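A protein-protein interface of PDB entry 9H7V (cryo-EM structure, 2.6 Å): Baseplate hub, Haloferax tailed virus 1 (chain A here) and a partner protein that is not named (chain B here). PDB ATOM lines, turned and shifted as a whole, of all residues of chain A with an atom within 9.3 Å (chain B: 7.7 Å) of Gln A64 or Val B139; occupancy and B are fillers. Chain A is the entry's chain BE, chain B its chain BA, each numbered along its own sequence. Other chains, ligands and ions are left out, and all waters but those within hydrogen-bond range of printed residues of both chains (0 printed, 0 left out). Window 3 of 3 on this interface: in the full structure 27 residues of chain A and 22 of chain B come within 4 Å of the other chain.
NH2 of Arg B137 lies within hydrogen-bond range of OD1 of Asn A37, 2.9 Å away.
The side-chain carboxylate (OE2) of Glu B196 is in salt-bridge range of the guanidinium group (NH1) of Arg A61 (2.8 Å).
O of Asp A60 is in hydrogen-bond range of NZ of Lys B198 (2.9 Å).
The side-chain amino group (NZ) of Lys B198 is in salt-bridge range of the side-chain carboxylate (OD2) of Asp A106 (2.8 Å).
O of Arg B137 lies within hydrogen-bond range of N of Val B197 (2.8 Å).
N of Asp A59 lies within hydrogen-bond range of O of Asn A37, at 3.1 Å.
The guanidinium group (NH2) of Arg A61 lies close to the side-chain amide nitrogen (ND2) of Asn A37.
OD1 of Asp A60 lies within hydrogen-bond range of N of Gln A64, at 3.0 Å.
N of Phe A66 is in hydrogen-bond range of OD2 of Asp A60 (3.0 Å).
The backbone NH (N) of Asp A60 sits at hydrogen-bond distance from the backbone carbonyl oxygen (O) of Asp A106, 3.1 Å away.
Glu B196 touches Asp A59.
NE of Arg A61 touches CB of Arg B137, at 3.5 Å.
CD of Arg A61 touches N of Gly B138, at 3.7 Å.
Arg A61 touches Val B139.
CG2 of Val B139 touches N of Gly A62, 3.7 Å away.
Gln A64 touches Val B139 (NE2 to CG2, 3.9 Å).
Gln A35 touches none of the printed residues of chain B.
Of the printed residues of chain B, Asp A60 touches Lys B198.
Printed residues of chain B within 4 Å of Arg A61: Arg B137, Gly B138, Val B139 and Glu B196.
Gly A63 touches none of the printed residues of chain B.
Gln A64 touches just one residue of chain B: Val B139 (3.9 Å).
Pro A70 touches none of the printed residues of chain B.
Printed residues of chain A within 4 Å of Gly B138: Arg A61.
Of chain A, only Arg A61 (3.6 Å), Gly A62 (3.7 Å) and Gln A64 (3.9 Å) come within 4 Å of Val B139.
Gly B140 touches none of the printed residues of chain A.
The nearest residue of chain A that does not touch Val B139 is Gly A63 (6.0 Å).
The nearest printed residue of chain A that does not touch Lys B198 is Arg A61 (4.3 Å).
Of the 13 printed residues of chain B, 5 touch a printed residue of chain A.
Hydrophobic or aromatic side chains of chain B within 4 Å of the printed part of chain A: Val B139.
Among the printed residues, Asp or Glu carboxylates within 4 Å of a Lys or Arg side-chain nitrogen of the other chain: Arg A61 with Glu B196 (2.8 Å) and Asp A106 with Lys B198 (2.8 Å).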
ATOM      1  N   GLU A  33      14.978 -19.996  33.371  1.00  0.00           N
ATOM      2  CA  GLU A  33      15.225 -20.021  31.930  1.00  0.00           C
ATOM      3  C   GLU A  33      15.930 -18.749  31.452  1.00  0.00           C
ATOM      4  O   GLU A  33      15.682 -17.666  31.980  1.00  0.00           O
ATOM      5  CB  GLU A  33      13.963 -20.382  31.137  1.00  0.00           C
ATOM      6  CG  GLU A  33      12.837 -19.362  31.209  1.00  0.00           C
ATOM      7  CD  GLU A  33      11.617 -19.708  30.369  1.00  0.00           C
ATOM      8  OE1 GLU A  33      11.127 -20.855  30.472  1.00  0.00           O
ATOM      9  OE2 GLU A  33      11.156 -18.831  29.610  1.00  0.00           O
ATOM     10  N   GLN A  35      17.131 -15.543  29.363  1.00  0.00           N
ATOM     11  CA  GLN A  35      16.632 -14.472  28.517  1.00  0.00           C
ATOM     12  C   GLN A  35      17.597 -14.285  27.348  1.00  0.00           C
ATOM     13  O   GLN A  35      18.807 -14.190  27.551  1.00  0.00           O
ATOM     14  CB  GLN A  35      16.457 -13.186  29.329  1.00  0.00           C
ATOM     15  CG  GLN A  35      15.723 -12.081  28.578  1.00  0.00           C
ATOM     16  CD  GLN A  35      14.314 -12.454  28.181  1.00  0.00           C
ATOM     17  OE1 GLN A  35      13.981 -12.523  27.001  1.00  0.00           O
ATOM     18  NE2 GLN A  35      13.472 -12.707  29.171  1.00  0.00           N
ATOM     19  N   ASN A  36      17.043 -14.216  26.131  1.00  0.00           N
ATOM     20  CA  ASN A  36      17.834 -14.211  24.910  1.00  0.00           C
ATOM     21  C   ASN A  36      18.358 -12.810  24.598  1.00  0.00           C
ATOM     22  O   ASN A  36      19.533 -12.654  24.268  1.00  0.00           O
ATOM     23  CB  ASN A  36      17.062 -14.758  23.705  1.00  0.00           C
ATOM     24  CG  ASN A  36      16.475 -16.136  23.924  1.00  0.00           C
ATOM     25  OD1 ASN A  36      15.257 -16.301  23.919  1.00  0.00           O
ATOM     26  ND2 ASN A  36      17.328 -17.131  24.117  1.00  0.00           N
ATOM     27  N   ASN A  37      17.484 -11.802  24.714  1.00  0.00           N
ATOM     28  CA  ASN A  37      17.657 -10.549  23.994  1.00  0.00           C
ATOM     29  C   ASN A  37      18.279  -9.467  24.882  1.00  0.00           C
ATOM     30  O   ASN A  37      17.973  -8.286  24.721  1.00  0.00           O
ATOM     31  CB  ASN A  37      16.348 -10.124  23.314  1.00  0.00           C
ATOM     32  CG  ASN A  37      15.728 -11.211  22.460  1.00  0.00           C
ATOM     33  OD1 ASN A  37      16.273 -11.579  21.421  1.00  0.00           O
ATOM     34  ND2 ASN A  37      14.582 -11.721  22.880  1.00  0.00           N
ATOM     35  N   ASP A  59      15.666  -6.292  24.586  1.00  0.00           N
ATOM     36  CA  ASP A  59      14.754  -5.987  23.496  1.00  0.00           C
ATOM     37  C   ASP A  59      13.525  -6.882  23.605  1.00  0.00           C
ATOM     38  O   ASP A  59      13.639  -8.080  23.861  1.00  0.00           O
ATOM     39  CB  ASP A  59      15.420  -6.170  22.132  1.00  0.00           C
ATOM     40  CG  ASP A  59      16.168  -4.943  21.642  1.00  0.00           C
ATOM     41  OD1 ASP A  59      15.518  -3.896  21.444  1.00  0.00           O
ATOM     42  OD2 ASP A  59      17.394  -5.045  21.463  1.00  0.00           O
ATOM     43  N   ASP A  60      12.355  -6.268  23.398  1.00  0.00           N
ATOM     44  CA  ASP A  60      11.074  -6.953  23.424  1.00  0.00           C
ATOM     45  C   ASP A  60      10.317  -6.651  22.132  1.00  0.00           C
ATOM     46  O   ASP A  60      10.667  -5.725  21.401  1.00  0.00           O
ATOM     47  CB  ASP A  60      10.282  -6.581  24.682  1.00  0.00           C
ATOM     48  CG  ASP A  60       9.201  -7.576  25.077  1.00  0.00           C
ATOM     49  OD1 ASP A  60       9.012  -8.576  24.351  1.00  0.00           O
ATOM     50  OD2 ASP A  60       8.562  -7.347  26.121  1.00  0.00           O
ATOM     51  N   ARG A  61       9.285  -7.462  21.865  1.00  0.00           N
ATOM     52  CA  ARG A  61       8.440  -7.359  20.686  1.00  0.00           C
ATOM     53  C   ARG A  61       7.058  -7.909  21.032  1.00  0.00           C
ATOM     54  O   ARG A  61       6.930  -9.064  21.437  1.00  0.00           O
ATOM     55  CB  ARG A  61       9.092  -8.071  19.491  1.00  0.00           C
ATOM     56  CG  ARG A  61       9.309  -9.568  19.673  1.00  0.00           C
ATOM     57  CD  ARG A  61      10.560 -10.130  19.025  1.00  0.00           C
ATOM     58  NE  ARG A  61      11.795  -9.543  19.538  1.00  0.00           N
ATOM     59  CZ  ARG A  61      12.353  -9.808  20.718  1.00  0.00           C
ATOM     60  NH1 ARG A  61      13.477  -9.204  21.059  1.00  0.00           N
ATOM     61  NH2 ARG A  61      11.791 -10.662  21.557  1.00  0.00           N
ATOM     62  N   GLY A  62       6.035  -7.055  20.905  1.00  0.00           N
ATOM     63  CA  GLY A  62       4.667  -7.408  21.259  1.00  0.00           C
ATOM     64  C   GLY A  62       4.490  -7.683  22.753  1.00  0.00           C
ATOM     65  O   GLY A  62       3.519  -8.327  23.147  1.00  0.00           O
ATOM     66  N   GLY A  63       5.445  -7.203  23.564  1.00  0.00           N
ATOM     67  CA  GLY A  63       5.396  -7.248  25.018  1.00  0.00           C
ATOM     68  C   GLY A  63       5.554  -8.654  25.597  1.00  0.00           C
ATOM     69  O   GLY A  63       5.124  -8.902  26.722  1.00  0.00           O
ATOM     70  N   GLN A  64       6.189  -9.552  24.833  1.00  0.00           N
ATOM     71  CA  GLN A  64       6.250 -10.971  25.157  1.00  0.00           C
ATOM     72  C   GLN A  64       7.205 -11.230  26.321  1.00  0.00           C
ATOM     73  O   GLN A  64       6.946 -12.113  27.138  1.00  0.00           O
ATOM     74  CB  GLN A  64       6.605 -11.794  23.917  1.00  0.00           C
ATOM     75  CG  GLN A  64       5.506 -11.811  22.862  1.00  0.00           C
ATOM     76  CD  GLN A  64       5.954 -12.325  21.513  1.00  0.00           C
ATOM     77  OE1 GLN A  64       7.033 -12.894  21.361  1.00  0.00           O
ATOM     78  NE2 GLN A  64       5.112 -12.130  20.512  1.00  0.00           N
ATOM     79  N   ALA A  65       8.296 -10.457  26.393  1.00  0.00           N
ATOM     80  CA  ALA A  65       9.298 -10.618  27.437  1.00  0.00           C
ATOM     81  C   ALA A  65       8.846  -9.970  28.746  1.00  0.00           C
ATOM     82  O   ALA A  65       9.220 -10.445  29.817  1.00  0.00           O
ATOM     83  CB  ALA A  65      10.633 -10.090  26.976  1.00  0.00           C
ATOM     84  N   PHE A  66       8.047  -8.897  28.651  1.00  0.00           N
ATOM     85  CA  PHE A  66       7.544  -8.147  29.798  1.00  0.00           C
ATOM     86  C   PHE A  66       6.734  -9.050  30.728  1.00  0.00           C
ATOM     87  O   PHE A  66       6.733  -8.840  31.940  1.00  0.00           O
ATOM     88  CB  PHE A  66       6.716  -6.949  29.317  1.00  0.00           C
ATOM     89  CG  PHE A  66       6.099  -6.063  30.375  1.00  0.00           C
ATOM     90  CD1 PHE A  66       6.837  -5.061  30.993  1.00  0.00           C
ATOM     91  CD2 PHE A  66       4.756  -6.189  30.711  1.00  0.00           C
ATOM     92  CE1 PHE A  66       6.258  -4.231  31.944  1.00  0.00           C
ATOM     93  CE2 PHE A  66       4.177  -5.357  31.661  1.00  0.00           C
ATOM     94  CZ  PHE A  66       4.930  -4.385  32.280  1.00  0.00           C
ATOM     95  N   GLU A  67       6.066 -10.055  30.146  1.00  0.00           N
ATOM     96  CA  GLU A  67       5.168 -10.949  30.864  1.00  0.00           C
ATOM     97  C   GLU A  67       5.948 -11.998  31.656  1.00  0.00           C
ATOM     98  O   GLU A  67       5.374 -12.669  32.511  1.00  0.00           O
ATOM     99  CB  GLU A  67       4.167 -11.597  29.903  1.00  0.00           C
ATOM    100  CG  GLU A  67       3.156 -10.627  29.308  1.00  0.00           C
ATOM    101  CD  GLU A  67       2.255  -9.874  30.278  1.00  0.00           C
ATOM    102  OE1 GLU A  67       1.887 -10.448  31.328  1.00  0.00           O
ATOM    103  OE2 GLU A  67       1.916  -8.711  29.977  1.00  0.00           O
ATOM    104  N   ALA A  68       7.252 -12.123  31.375  1.00  0.00           N
ATOM    105  CA  ALA A  68       8.096 -13.128  32.002  1.00  0.00           C
ATOM    106  C   ALA A  68       8.609 -12.657  33.363  1.00  0.00           C
ATOM    107  O   ALA A  68       9.122 -13.467  34.134  1.00  0.00           O
ATOM    108  CB  ALA A  68       9.232 -13.500  31.080  1.00  0.00           C
ATOM    109  N   TYR A  69       8.440 -11.361  33.667  1.00  0.00           N
ATOM    110  CA  TYR A  69       9.086 -10.758  34.823  1.00  0.00           C
ATOM    111  C   TYR A  69       8.092 -10.152  35.822  1.00  0.00           C
ATOM    112  O   TYR A  69       8.321  -9.025  36.261  1.00  0.00           O
ATOM    113  CB  TYR A  69      10.062  -9.670  34.365  1.00  0.00           C
ATOM    114  CG  TYR A  69      11.289 -10.125  33.615  1.00  0.00           C
ATOM    115  CD1 TYR A  69      12.450 -10.476  34.291  1.00  0.00           C
ATOM    116  CD2 TYR A  69      11.309 -10.156  32.229  1.00  0.00           C
ATOM    117  CE1 TYR A  69      13.591 -10.868  33.607  1.00  0.00           C
ATOM    118  CE2 TYR A  69      12.438 -10.553  31.529  1.00  0.00           C
ATOM    119  CZ  TYR A  69      13.580 -10.913  32.223  1.00  0.00           C
ATOM    120  OH  TYR A  69      14.698 -11.298  31.544  1.00  0.00           O
ATOM    121  N   PRO A  70       7.004 -10.837  36.273  1.00  0.00           N
ATOM    122  CA  PRO A  70       6.169 -10.316  37.365  1.00  0.00           C
ATOM    123  C   PRO A  70       6.966  -9.994  38.629  1.00  0.00           C
ATOM    124  O   PRO A  70       8.036 -10.560  38.844  1.00  0.00           O
ATOM    125  CB  PRO A  70       5.202 -11.467  37.672  1.00  0.00           C
ATOM    126  CG  PRO A  70       5.104 -12.226  36.373  1.00  0.00           C
ATOM    127  CD  PRO A  70       6.484 -12.117  35.760  1.00  0.00           C
ATOM    128  N   ARG A  97       9.460  -3.793  36.403  1.00  0.00           N
ATOM    129  CA  ARG A  97       9.553  -4.073  34.978  1.00  0.00           C
ATOM    130  C   ARG A  97       9.006  -2.865  34.222  1.00  0.00           C
ATOM    131  O   ARG A  97       7.874  -2.448  34.456  1.00  0.00           O
ATOM    132  CB  ARG A  97       8.834  -5.381  34.613  1.00  0.00           C
ATOM    133  CG  ARG A  97       7.385  -5.483  35.074  1.00  0.00           C
ATOM    134  CD  ARG A  97       6.801  -6.882  35.010  1.00  0.00           C
ATOM    135  NE  ARG A  97       5.742  -7.166  34.049  1.00  0.00           N
ATOM    136  CZ  ARG A  97       4.553  -7.687  34.353  1.00  0.00           C
ATOM    137  NH1 ARG A  97       3.668  -7.920  33.400  1.00  0.00           N
ATOM    138  NH2 ARG A  97       4.249  -7.985  35.604  1.00  0.00           N
ATOM    139  N   GLU A  99       8.850  -0.873  30.247  1.00  0.00           N
ATOM    140  CA  GLU A  99       9.071  -0.922  28.812  1.00  0.00           C
ATOM    141  C   GLU A  99       8.695   0.414  28.180  1.00  0.00           C
ATOM    142  O   GLU A  99       7.612   0.941  28.429  1.00  0.00           O
ATOM    143  CB  GLU A  99       8.304  -2.082  28.181  1.00  0.00           C
ATOM    144  CG  GLU A  99       8.862  -2.500  26.831  1.00  0.00           C
ATOM    145  CD  GLU A  99       8.140  -3.652  26.153  1.00  0.00           C
ATOM    146  OE1 GLU A  99       7.517  -4.470  26.864  1.00  0.00           O
ATOM    147  OE2 GLU A  99       8.205  -3.731  24.911  1.00  0.00           O
ATOM    148  N   ASP A 106      11.766  -1.104  21.359  1.00  0.00           N
ATOM    149  CA  ASP A 106      10.936  -1.429  22.509  1.00  0.00           C
ATOM    150  C   ASP A 106      11.840  -2.035  23.579  1.00  0.00           C
ATOM    151  O   ASP A 106      12.201  -3.209  23.499  1.00  0.00           O
ATOM    152  CB  ASP A 106       9.787  -2.368  22.126  1.00  0.00           C
ATOM    153  CG  ASP A 106       8.929  -1.874  20.972  1.00  0.00           C
ATOM    154  OD1 ASP A 106       8.294  -0.812  21.121  1.00  0.00           O
ATOM    155  OD2 ASP A 106       8.901  -2.560  19.934  1.00  0.00           O
ATOM    156  N   LEU A 108      12.919  -3.234  27.206  1.00  0.00           N
ATOM    157  CA  LEU A 108      12.517  -3.762  28.498  1.00  0.00           C
ATOM    158  C   LEU A 108      13.662  -3.574  29.489  1.00  0.00           C
ATOM    159  O   LEU A 108      14.763  -4.078  29.277  1.00  0.00           O
ATOM    160  CB  LEU A 108      12.120  -5.236  28.347  1.00  0.00           C
ATOM    161  CG  LEU A 108      11.834  -6.003  29.640  1.00  0.00           C
ATOM    162  CD1 LEU A 108      10.611  -5.455  30.364  1.00  0.00           C
ATOM    163  CD2 LEU A 108      11.656  -7.485  29.362  1.00  0.00           C
ATOM    164  N   ALA B  80       8.054  -3.660   6.417  1.00  0.00           N
ATOM    165  CA  ALA B  80       8.348  -4.322   7.677  1.00  0.00           C
ATOM    166  C   ALA B  80       7.882  -5.773   7.592  1.00  0.00           C
ATOM    167  O   ALA B  80       6.684  -6.032   7.492  1.00  0.00           O
ATOM    168  CB  ALA B  80       7.670  -3.592   8.812  1.00  0.00           C
ATOM    169  N   SER B  81       8.844  -6.704   7.597  1.00  0.00           N
ATOM    170  CA  SER B  81       8.563  -8.132   7.620  1.00  0.00           C
ATOM    171  C   SER B  81       9.717  -8.886   8.272  1.00  0.00           C
ATOM    172  O   SER B  81      10.878  -8.508   8.116  1.00  0.00           O
ATOM    173  CB  SER B  81       8.270  -8.669   6.239  1.00  0.00           C
ATOM    174  OG  SER B  81       7.791 -10.005   6.308  1.00  0.00           O
ATOM    175  N   THR B  82       9.372  -9.968   8.982  1.00  0.00           N
ATOM    176  CA  THR B  82      10.335 -10.796   9.691  1.00  0.00           C
ATOM    177  C   THR B  82      10.873 -11.907   8.789  1.00  0.00           C
ATOM    178  O   THR B  82      11.722 -12.687   9.221  1.00  0.00           O
ATOM    179  CB  THR B  82       9.758 -11.351  10.999  1.00  0.00           C
ATOM    180  OG1 THR B  82       8.561 -12.068  10.703  1.00  0.00           O
ATOM    181  CG2 THR B  82       9.473 -10.272  12.019  1.00  0.00           C
ATOM    182  N   ARG B 137      14.011 -10.732  14.329  1.00  0.00           N
ATOM    183  CA  ARG B 137      12.998 -10.845  15.368  1.00  0.00           C
ATOM    184  C   ARG B 137      11.935  -9.767  15.164  1.00  0.00           C
ATOM    185  O   ARG B 137      12.268  -8.631  14.830  1.00  0.00           O
ATOM    186  CB  ARG B 137      13.648 -10.670  16.746  1.00  0.00           C
ATOM    187  CG  ARG B 137      14.762 -11.660  17.060  1.00  0.00           C
ATOM    188  CD  ARG B 137      14.299 -12.889  17.819  1.00  0.00           C
ATOM    189  NE  ARG B 137      15.205 -14.016  17.634  1.00  0.00           N
ATOM    190  CZ  ARG B 137      16.341 -14.219  18.300  1.00  0.00           C
ATOM    191  NH1 ARG B 137      17.072 -15.287  18.033  1.00  0.00           N
ATOM    192  NH2 ARG B 137      16.748 -13.364  19.222  1.00  0.00           N
ATOM    193  N   GLY B 138      10.660 -10.128  15.375  1.00  0.00           N
ATOM    194  CA  GLY B 138       9.579  -9.152  15.320  1.00  0.00           C
ATOM    195  C   GLY B 138       8.179  -9.764  15.319  1.00  0.00           C
ATOM    196  O   GLY B 138       8.023 -10.984  15.351  1.00  0.00           O
ATOM    197  N   VAL B 139       7.172  -8.881  15.265  1.00  0.00           N
ATOM    198  CA  VAL B 139       5.769  -9.248  15.392  1.00  0.00           C
ATOM    199  C   VAL B 139       5.020  -8.915  14.100  1.00  0.00           C
ATOM    200  O   VAL B 139       4.333  -9.777  13.553  1.00  0.00           O
ATOM    201  CB  VAL B 139       5.121  -8.614  16.644  1.00  0.00           C
ATOM    202  CG1 VAL B 139       3.600  -8.714  16.639  1.00  0.00           C
ATOM    203  CG2 VAL B 139       5.680  -9.199  17.932  1.00  0.00           C
ATOM    204  N   GLY B 140       5.172  -7.677  13.608  1.00  0.00           N
ATOM    205  CA  GLY B 140       4.261  -7.117  12.620  1.00  0.00           C
ATOM    206  C   GLY B 140       4.742  -7.244  11.177  1.00  0.00           C
ATOM    207  O   GLY B 140       5.938  -7.168  10.902  1.00  0.00           O
ATOM    208  N   ASP B 141       3.773  -7.441  10.272  1.00  0.00           N
ATOM    209  CA  ASP B 141       3.948  -7.282   8.837  1.00  0.00           C
ATOM    210  C   ASP B 141       3.269  -5.986   8.404  1.00  0.00           C
ATOM    211  O   ASP B 141       2.085  -5.783   8.676  1.00  0.00           O
ATOM    212  CB  ASP B 141       3.355  -8.458   8.055  1.00  0.00           C
ATOM    213  CG  ASP B 141       4.218  -9.709   8.036  1.00  0.00           C
ATOM    214  OD1 ASP B 141       5.399  -9.608   7.649  1.00  0.00           O
ATOM    215  OD2 ASP B 141       3.695 -10.781   8.402  1.00  0.00           O
ATOM    216  N   GLN B 142       4.039  -5.115   7.743  1.00  0.00           N
ATOM    217  CA  GLN B 142       3.501  -3.935   7.083  1.00  0.00           C
ATOM    218  C   GLN B 142       4.032  -3.887   5.653  1.00  0.00           C
ATOM    219  O   GLN B 142       5.205  -3.594   5.426  1.00  0.00           O
ATOM    220  CB  GLN B 142       3.793  -2.661   7.881  1.00  0.00           C
ATOM    221  CG  GLN B 142       3.019  -2.575   9.191  1.00  0.00           C
ATOM    222  CD  GLN B 142       3.005  -1.212   9.840  1.00  0.00           C
ATOM    223  OE1 GLN B 142       3.927  -0.412   9.690  1.00  0.00           O
ATOM    224  NE2 GLN B 142       1.949  -0.942  10.590  1.00  0.00           N
ATOM    225  N   GLU B 196      15.816  -6.248  14.988  1.00  0.00           N
ATOM    226  CA  GLU B 196      14.477  -6.081  15.529  1.00  0.00           C
ATOM    227  C   GLU B 196      13.637  -5.317  14.508  1.00  0.00           C
ATOM    228  O   GLU B 196      13.797  -4.108  14.345  1.00  0.00           O
ATOM    229  CB  GLU B 196      14.509  -5.354  16.877  1.00  0.00           C
ATOM    230  CG  GLU B 196      15.267  -6.090  17.972  1.00  0.00           C
ATOM    231  CD  GLU B 196      14.598  -7.312  18.584  1.00  0.00           C
ATOM    232  OE1 GLU B 196      13.368  -7.466  18.433  1.00  0.00           O
ATOM    233  OE2 GLU B 196      15.313  -8.110  19.220  1.00  0.00           O
ATOM    234  N   VAL B 197      12.762  -6.052  13.811  1.00  0.00           N
ATOM    235  CA  VAL B 197      11.851  -5.483  12.829  1.00  0.00           C
ATOM    236  C   VAL B 197      10.685  -4.844  13.582  1.00  0.00           C
ATOM    237  O   VAL B 197      10.012  -5.510  14.366  1.00  0.00           O
ATOM    238  CB  VAL B 197      11.365  -6.543  11.818  1.00  0.00           C
ATOM    239  CG1 VAL B 197      10.390  -5.967  10.800  1.00  0.00           C
ATOM    240  CG2 VAL B 197      12.517  -7.236  11.108  1.00  0.00           C
ATOM    241  N   LYS B 198      10.460  -3.550  13.322  1.00  0.00           N
ATOM    242  CA  LYS B 198       9.430  -2.781  14.004  1.00  0.00           C
ATOM    243  C   LYS B 198       8.381  -2.315  12.999  1.00  0.00           C
ATOM    244  O   LYS B 198       8.715  -1.699  11.990  1.00  0.00           O
ATOM    245  CB  LYS B 198      10.045  -1.593  14.753  1.00  0.00           C
ATOM    246  CG  LYS B 198      11.045  -1.939  15.850  1.00  0.00           C
ATOM    247  CD  LYS B 198      10.476  -2.827  16.940  1.00  0.00           C
ATOM    248  CE  LYS B 198      11.497  -3.218  17.984  1.00  0.00           C
ATOM    249  NZ  LYS B 198      10.942  -4.209  18.936  1.00  0.00           N
ATOM    250  N   ALA B 199       7.110  -2.612  13.302  1.00  0.00           N
ATOM    251  CA  ALA B 199       5.980  -2.125  12.528  1.00  0.00           C
ATOM    252  C   ALA B 199       5.686  -0.677  12.922  1.00  0.00           C
ATOM    253  O   ALA B 199       4.650  -0.379  13.518  1.00  0.00           O
ATOM    254  CB  ALA B 199       4.789  -3.034  12.725  1.00  0.00           C
